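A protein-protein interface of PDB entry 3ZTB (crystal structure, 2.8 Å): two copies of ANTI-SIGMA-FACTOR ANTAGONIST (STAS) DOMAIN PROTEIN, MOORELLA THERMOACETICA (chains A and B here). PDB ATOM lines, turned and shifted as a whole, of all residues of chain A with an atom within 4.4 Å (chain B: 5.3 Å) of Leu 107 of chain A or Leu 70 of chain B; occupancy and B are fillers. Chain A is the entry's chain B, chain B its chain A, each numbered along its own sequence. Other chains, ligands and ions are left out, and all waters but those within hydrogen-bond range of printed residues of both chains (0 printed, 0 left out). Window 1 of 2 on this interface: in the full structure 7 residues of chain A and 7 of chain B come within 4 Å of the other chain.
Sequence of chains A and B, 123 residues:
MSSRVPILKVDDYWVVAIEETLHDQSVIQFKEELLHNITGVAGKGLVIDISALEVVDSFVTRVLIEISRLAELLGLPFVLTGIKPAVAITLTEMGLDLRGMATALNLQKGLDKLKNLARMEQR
Of chain B, only Leu 70 (3.5 Å), Leu 73 (3.5 Å) and Leu 74 (3.8 Å) come within 4 Å of Leu 107 of chain A. Leu 70 of chain B touches just these residues of chain A: Leu 8 (3.6 Å) and Leu 107 (3.5 Å). Of the printed residues of chain A, Glu 66 of chain B touches Leu 8. Of the printed residues of chain A, Leu 73 of chain B touches Leu 8, Asp 49 and Leu 107. Of the printed residues of chain A, Leu 74 of chain B touches Leu 107 and Gln 108. Of the printed residues of chain B, Gln 108 of chain A touches Leu 74. Ile 65 of chain B touches none of the printed residues of chain A. The nearest printed residue of chain B that does not touch Leu 107 of chain A is Arg 69 of chain B (6.0 Å). The nearest printed residue of chain A that does not touch Leu 70 of chain B is Val 15 of chain A (4.7 Å).
No position is printed for both chains. Of the 8 pairs that touch across the chains among the printed residues, none has its exchanged pair printed and touching as well.
Among the printed residues, pairs that only touch across the chains: Leu 8 of chain A with Glu 66 of chain B (3.8 Å), Leu 8 of chain A with Leu 70 of chain B (3.6 Å), Leu 8 of chain A with Leu 73 of chain B (3.6 Å), Asp 49 of chain A with Leu 73 of chain B (3.3 Å), Leu 107 of chain A with Leu 70 of chain B (3.5 Å), Leu 107 of chain A with Leu 73 of chain B (3.5 Å), Leu 107 of chain A with Leu 74 of chain B (3.8 Å) and Gln 108 of chain A with Leu 74 of chain B (3.8 Å).
Of the 12 printed residues of chain B, 4 touch a printed residue of chain A. Among the printed residues, 8 pairs touch across the chains. Among the printed residues, no Asp or Glu carboxylate lies within 4 Å of a Lys or Arg side-chain nitrogen of the other chain.
The side-chain amide oxygen (OD1) of Asn 106 of chain A sits close to the backbone NH (N) of Gln 108 of chain A, 3.5 Å away. The backbone NH of Val 15 of chain A lies within hydrogen-bond range of the backbone carbonyl oxygen of Leu 8 of chain A (2.9 Å). OD1 of Asp 49 of chain A sits at hydrogen-bond distance from OG1 of Thr 81 of chain A.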
ATOM      1  N   LEU A   8     -21.208   0.380 -11.568  1.00  0.00           N
ATOM      2  CA  LEU A   8     -21.144   1.704 -12.175  1.00  0.00           C
ATOM      3  C   LEU A   8     -22.077   2.676 -11.442  1.00  0.00           C
ATOM      4  O   LEU A   8     -22.943   2.253 -10.673  1.00  0.00           O
ATOM      5  CB  LEU A   8     -21.509   1.619 -13.657  1.00  0.00           C
ATOM      6  CG  LEU A   8     -20.817   0.506 -14.442  1.00  0.00           C
ATOM      7  CD1 LEU A   8     -21.490   0.271 -15.785  1.00  0.00           C
ATOM      8  CD2 LEU A   8     -19.337   0.805 -14.636  1.00  0.00           C
ATOM      9  N   VAL A  15     -25.694   1.600 -11.067  1.00  0.00           N
ATOM     10  CA  VAL A  15     -25.957   0.756 -12.227  1.00  0.00           C
ATOM     11  C   VAL A  15     -25.234  -0.580 -12.121  1.00  0.00           C
ATOM     12  O   VAL A  15     -24.004  -0.631 -12.128  1.00  0.00           O
ATOM     13  CB  VAL A  15     -25.526   1.435 -13.537  1.00  0.00           C
ATOM     14  CG1 VAL A  15     -25.825   0.536 -14.731  1.00  0.00           C
ATOM     15  CG2 VAL A  15     -26.220   2.778 -13.692  1.00  0.00           C
ATOM     16  N   VAL A  47     -30.330   1.021 -11.369  1.00  0.00           N
ATOM     17  CA  VAL A  47     -30.639   0.431 -12.664  1.00  0.00           C
ATOM     18  C   VAL A  47     -29.907  -0.897 -12.805  1.00  0.00           C
ATOM     19  O   VAL A  47     -28.689  -0.958 -12.649  1.00  0.00           O
ATOM     20  CB  VAL A  47     -30.223   1.349 -13.826  1.00  0.00           C
ATOM     21  CG1 VAL A  47     -30.597   0.720 -15.164  1.00  0.00           C
ATOM     22  CG2 VAL A  47     -30.861   2.722 -13.682  1.00  0.00           C
ATOM     23  N   ASP A  49     -29.041  -3.723 -15.546  1.00  0.00           N
ATOM     24  CA  ASP A  49     -29.055  -3.999 -16.973  1.00  0.00           C
ATOM     25  C   ASP A  49     -28.730  -5.467 -17.232  1.00  0.00           C
ATOM     26  O   ASP A  49     -27.693  -5.969 -16.800  1.00  0.00           O
ATOM     27  CB  ASP A  49     -28.069  -3.082 -17.703  1.00  0.00           C
ATOM     28  CG  ASP A  49     -28.355  -2.978 -19.188  1.00  0.00           C
ATOM     29  OD1 ASP A  49     -29.375  -2.359 -19.558  1.00  0.00           O
ATOM     30  OD2 ASP A  49     -27.553  -3.504 -19.987  1.00  0.00           O
ATOM     31  N   THR A  81     -33.577  -3.032 -16.858  1.00  0.00           N
ATOM     32  CA  THR A  81     -33.413  -2.612 -18.245  1.00  0.00           C
ATOM     33  C   THR A  81     -32.696  -3.648 -19.101  1.00  0.00           C
ATOM     34  O   THR A  81     -31.872  -4.416 -18.603  1.00  0.00           O
ATOM     35  CB  THR A  81     -32.642  -1.286 -18.343  1.00  0.00           C
ATOM     36  OG1 THR A  81     -31.304  -1.465 -17.865  1.00  0.00           O
ATOM     37  CG2 THR A  81     -33.327  -0.202 -17.524  1.00  0.00           C
ATOM     38  N   ASN A 106     -33.208   0.330 -22.344  1.00  0.00           N
ATOM     39  CA  ASN A 106     -31.767   0.339 -22.115  1.00  0.00           C
ATOM     40  C   ASN A 106     -31.378   1.220 -20.928  1.00  0.00           C
ATOM     41  O   ASN A 106     -32.244   1.757 -20.240  1.00  0.00           O
ATOM     42  CB  ASN A 106     -31.014   0.746 -23.389  1.00  0.00           C
ATOM     43  CG  ASN A 106     -31.668   1.904 -24.118  1.00  0.00           C
ATOM     44  OD1 ASN A 106     -32.127   2.863 -23.502  1.00  0.00           O
ATOM     45  ND2 ASN A 106     -31.716   1.814 -25.445  1.00  0.00           N
ATOM     46  N   LEU A 107     -30.082   1.359 -20.679  1.00  0.00           N
ATOM     47  CA  LEU A 107     -29.613   2.164 -19.552  1.00  0.00           C
ATOM     48  C   LEU A 107     -30.138   3.599 -19.614  1.00  0.00           C
ATOM     49  O   LEU A 107     -30.430   4.209 -18.585  1.00  0.00           O
ATOM     50  CB  LEU A 107     -28.085   2.169 -19.492  1.00  0.00           C
ATOM     51  CG  LEU A 107     -27.459   3.133 -18.486  1.00  0.00           C
ATOM     52  CD1 LEU A 107     -27.811   2.728 -17.064  1.00  0.00           C
ATOM     53  CD2 LEU A 107     -25.952   3.199 -18.664  1.00  0.00           C
ATOM     54  N   GLN A 108     -30.260   4.125 -20.830  1.00  0.00           N
ATOM     55  CA  GLN A 108     -30.655   5.515 -21.057  1.00  0.00           C
ATOM     56  C   GLN A 108     -32.125   5.777 -20.735  1.00  0.00           C
ATOM     57  O   GLN A 108     -32.448   6.696 -19.983  1.00  0.00           O
ATOM     58  CB  GLN A 108     -30.378   5.910 -22.509  1.00  0.00           C
ATOM     59  CG  GLN A 108     -30.646   7.374 -22.823  1.00  0.00           C
ATOM     60  CD  GLN A 108     -29.447   8.259 -22.544  1.00  0.00           C
ATOM     61  OE1 GLN A 108     -29.385   8.935 -21.518  1.00  0.00           O
ATOM     62  NE2 GLN A 108     -28.487   8.261 -23.462  1.00  0.00           N
ATOM     63  N   LYS A 109     -33.014   4.980 -21.321  1.00  0.00           N
ATOM     64  CA  LYS A 109     -34.444   5.159 -21.111  1.00  0.00           C
ATOM     65  C   LYS A 109     -34.786   4.941 -19.647  1.00  0.00           C
ATOM     66  O   LYS A 109     -35.654   5.614 -19.096  1.00  0.00           O
ATOM     67  CB  LYS A 109     -35.237   4.190 -21.985  1.00  0.00           C
ATOM     68  CG  LYS A 109     -34.914   4.283 -23.467  1.00  0.00           C
ATOM     69  CD  LYS A 109     -35.891   5.186 -24.198  1.00  0.00           C
ATOM     70  CE  LYS A 109     -37.183   4.449 -24.504  1.00  0.00           C
ATOM     71  NZ  LYS A 109     -38.384   5.268 -24.192  1.00  0.00           N
ATOM     72  N   GLY A 110     -34.094   3.990 -19.027  1.00  0.00           N
ATOM     73  CA  GLY A 110     -34.263   3.709 -17.615  1.00  0.00           C
ATOM     74  C   GLY A 110     -33.811   4.872 -16.754  1.00  0.00           C
ATOM     75  O   GLY A 110     -34.491   5.245 -15.799  1.00  0.00           O
ATOM     76  N   LEU A 111     -32.659   5.446 -17.089  1.00  0.00           N
ATOM     77  CA  LEU A 111     -32.170   6.620 -16.376  1.00  0.00           C
ATOM     78  C   LEU A 111     -33.157   7.771 -16.527  1.00  0.00           C
ATOM     79  O   LEU A 111     -33.418   8.508 -15.576  1.00  0.00           O
ATOM     80  CB  LEU A 111     -30.782   7.032 -16.874  1.00  0.00           C
ATOM     81  CG  LEU A 111     -29.593   6.222 -16.351  1.00  0.00           C
ATOM     82  CD1 LEU A 111     -28.312   6.615 -17.073  1.00  0.00           C
ATOM     83  CD2 LEU A 111     -29.435   6.396 -14.847  1.00  0.00           C
ATOM     84  N   LEU B  35     -20.163  11.909 -17.476  1.00  0.00           N
ATOM     85  CA  LEU B  35     -21.275  10.962 -17.452  1.00  0.00           C
ATOM     86  C   LEU B  35     -22.631  11.655 -17.322  1.00  0.00           C
ATOM     87  O   LEU B  35     -23.655  11.105 -17.723  1.00  0.00           O
ATOM     88  CB  LEU B  35     -21.087   9.940 -16.327  1.00  0.00           C
ATOM     89  CG  LEU B  35     -19.854   9.050 -16.484  1.00  0.00           C
ATOM     90  CD1 LEU B  35     -19.623   8.201 -15.244  1.00  0.00           C
ATOM     91  CD2 LEU B  35     -20.004   8.181 -17.719  1.00  0.00           C
ATOM     92  N   ILE B  65     -12.153   2.866 -17.318  1.00  0.00           N
ATOM     93  CA  ILE B  65     -12.911   1.639 -17.541  1.00  0.00           C
ATOM     94  C   ILE B  65     -14.392   1.912 -17.331  1.00  0.00           C
ATOM     95  O   ILE B  65     -15.241   1.424 -18.078  1.00  0.00           O
ATOM     96  CB  ILE B  65     -12.474   0.500 -16.600  1.00  0.00           C
ATOM     97  CG1 ILE B  65     -11.048   0.049 -16.920  1.00  0.00           C
ATOM     98  CG2 ILE B  65     -13.420  -0.684 -16.720  1.00  0.00           C
ATOM     99  CD1 ILE B  65     -10.629  -1.211 -16.187  1.00  0.00           C
ATOM    100  N   GLU B  66     -14.687   2.705 -16.309  1.00  0.00           N
ATOM    101  CA  GLU B  66     -16.055   3.036 -15.937  1.00  0.00           C
ATOM    102  C   GLU B  66     -16.783   3.769 -17.063  1.00  0.00           C
ATOM    103  O   GLU B  66     -17.972   3.550 -17.290  1.00  0.00           O
ATOM    104  CB  GLU B  66     -16.052   3.874 -14.657  1.00  0.00           C
ATOM    105  CG  GLU B  66     -17.413   4.069 -14.024  1.00  0.00           C
ATOM    106  CD  GLU B  66     -17.321   4.569 -12.595  1.00  0.00           C
ATOM    107  OE1 GLU B  66     -16.213   4.531 -12.020  1.00  0.00           O
ATOM    108  OE2 GLU B  66     -18.357   4.999 -12.048  1.00  0.00           O
ATOM    109  N   ILE B  67     -16.060   4.634 -17.768  1.00  0.00           N
ATOM    110  CA  ILE B  67     -16.637   5.386 -18.878  1.00  0.00           C
ATOM    111  C   ILE B  67     -16.751   4.523 -20.133  1.00  0.00           C
ATOM    112  O   ILE B  67     -17.658   4.711 -20.941  1.00  0.00           O
ATOM    113  CB  ILE B  67     -15.820   6.659 -19.185  1.00  0.00           C
ATOM    114  CG1 ILE B  67     -15.669   7.505 -17.918  1.00  0.00           C
ATOM    115  CG2 ILE B  67     -16.479   7.464 -20.297  1.00  0.00           C
ATOM    116  CD1 ILE B  67     -14.740   8.686 -18.075  1.00  0.00           C
ATOM    117  N   SER B  68     -15.835   3.572 -20.291  1.00  0.00           N
ATOM    118  CA  SER B  68     -15.872   2.669 -21.436  1.00  0.00           C
ATOM    119  C   SER B  68     -17.069   1.729 -21.332  1.00  0.00           C
ATOM    120  O   SER B  68     -17.728   1.430 -22.329  1.00  0.00           O
ATOM    121  CB  SER B  68     -14.576   1.861 -21.531  1.00  0.00           C
ATOM    122  OG  SER B  68     -14.637   0.689 -20.737  1.00  0.00           O
ATOM    123  N   ARG B  69     -17.347   1.276 -20.114  1.00  0.00           N
ATOM    124  CA  ARG B  69     -18.459   0.367 -19.856  1.00  0.00           C
ATOM    125  C   ARG B  69     -19.821   1.059 -19.887  1.00  0.00           C
ATOM    126  O   ARG B  69     -20.828   0.436 -20.217  1.00  0.00           O
ATOM    127  CB  ARG B  69     -18.277  -0.347 -18.514  1.00  0.00           C
ATOM    128  CG  ARG B  69     -17.351  -1.547 -18.557  1.00  0.00           C
ATOM    129  CD  ARG B  69     -17.357  -2.268 -17.222  1.00  0.00           C
ATOM    130  NE  ARG B  69     -16.055  -2.851 -16.916  1.00  0.00           N
ATOM    131  CZ  ARG B  69     -15.698  -4.090 -17.230  1.00  0.00           C
ATOM    132  NH1 ARG B  69     -16.550  -4.889 -17.859  1.00  0.00           N
ATOM    133  NH2 ARG B  69     -14.489  -4.534 -16.912  1.00  0.00           N
ATOM    134  N   LEU B  70     -19.858   2.341 -19.536  1.00  0.00           N
ATOM    135  CA  LEU B  70     -21.120   3.076 -19.527  1.00  0.00           C
ATOM    136  C   LEU B  70     -21.514   3.581 -20.911  1.00  0.00           C
ATOM    137  O   LEU B  70     -22.701   3.690 -21.218  1.00  0.00           O
ATOM    138  CB  LEU B  70     -21.088   4.229 -18.522  1.00  0.00           C
ATOM    139  CG  LEU B  70     -21.433   3.836 -17.083  1.00  0.00           C
ATOM    140  CD1 LEU B  70     -21.177   4.989 -16.126  1.00  0.00           C
ATOM    141  CD2 LEU B  70     -22.876   3.361 -16.984  1.00  0.00           C
ATOM    142  N   ALA B  71     -20.524   3.892 -21.739  1.00  0.00           N
ATOM    143  CA  ALA B  71     -20.796   4.300 -23.109  1.00  0.00           C
ATOM    144  C   ALA B  71     -21.261   3.094 -23.910  1.00  0.00           C
ATOM    145  O   ALA B  71     -22.117   3.207 -24.784  1.00  0.00           O
ATOM    146  CB  ALA B  71     -19.560   4.908 -23.734  1.00  0.00           C
ATOM    147  N   GLU B  72     -20.685   1.937 -23.602  1.00  0.00           N
ATOM    148  CA  GLU B  72     -21.093   0.684 -24.221  1.00  0.00           C
ATOM    149  C   GLU B  72     -22.545   0.388 -23.862  1.00  0.00           C
ATOM    150  O   GLU B  72     -23.260  -0.282 -24.608  1.00  0.00           O
ATOM    151  CB  GLU B  72     -20.186  -0.452 -23.744  1.00  0.00           C
ATOM    152  CG  GLU B  72     -20.594  -1.836 -24.219  1.00  0.00           C
ATOM    153  CD  GLU B  72     -20.263  -2.081 -25.678  1.00  0.00           C
ATOM    154  OE1 GLU B  72     -19.064  -2.230 -25.999  1.00  0.00           O
ATOM    155  OE2 GLU B  72     -21.197  -2.127 -26.504  1.00  0.00           O
ATOM    156  N   LEU B  73     -22.971   0.904 -22.714  1.00  0.00           N
ATOM    157  CA  LEU B  73     -24.339   0.722 -22.239  1.00  0.00           C
ATOM    158  C   LEU B  73     -25.289   1.767 -22.819  1.00  0.00           C
ATOM    159  O   LEU B  73     -26.500   1.559 -22.868  1.00  0.00           O
ATOM    160  CB  LEU B  73     -24.385   0.763 -20.709  1.00  0.00           C
ATOM    161  CG  LEU B  73     -23.876  -0.475 -19.969  1.00  0.00           C
ATOM    162  CD1 LEU B  73     -23.805  -0.218 -18.471  1.00  0.00           C
ATOM    163  CD2 LEU B  73     -24.768  -1.665 -20.270  1.00  0.00           C
ATOM    164  N   LEU B  74     -24.731   2.890 -23.260  1.00  0.00           N
ATOM    165  CA  LEU B  74     -25.529   3.971 -23.826  1.00  0.00           C
ATOM    166  C   LEU B  74     -25.493   3.944 -25.351  1.00  0.00           C
ATOM    167  O   LEU B  74     -26.119   4.775 -26.010  1.00  0.00           O
ATOM    168  CB  LEU B  74     -25.034   5.324 -23.312  1.00  0.00           C
ATOM    169  CG  LEU B  74     -25.142   5.574 -21.808  1.00  0.00           C
ATOM    170  CD1 LEU B  74     -24.297   6.770 -21.397  1.00  0.00           C
ATOM    171  CD2 LEU B  74     -26.593   5.769 -21.393  1.00  0.00           C
ATOM    172  N   GLY B  75     -24.760   2.981 -25.902  1.00  0.00           N
ATOM    173  CA  GLY B  75     -24.600   2.866 -27.339  1.00  0.00           C
ATOM    174  C   GLY B  75     -23.779   4.013 -27.889  1.00  0.00           C
ATOM    175  O   GLY B  75     -24.001   4.477 -29.007  1.00  0.00           O
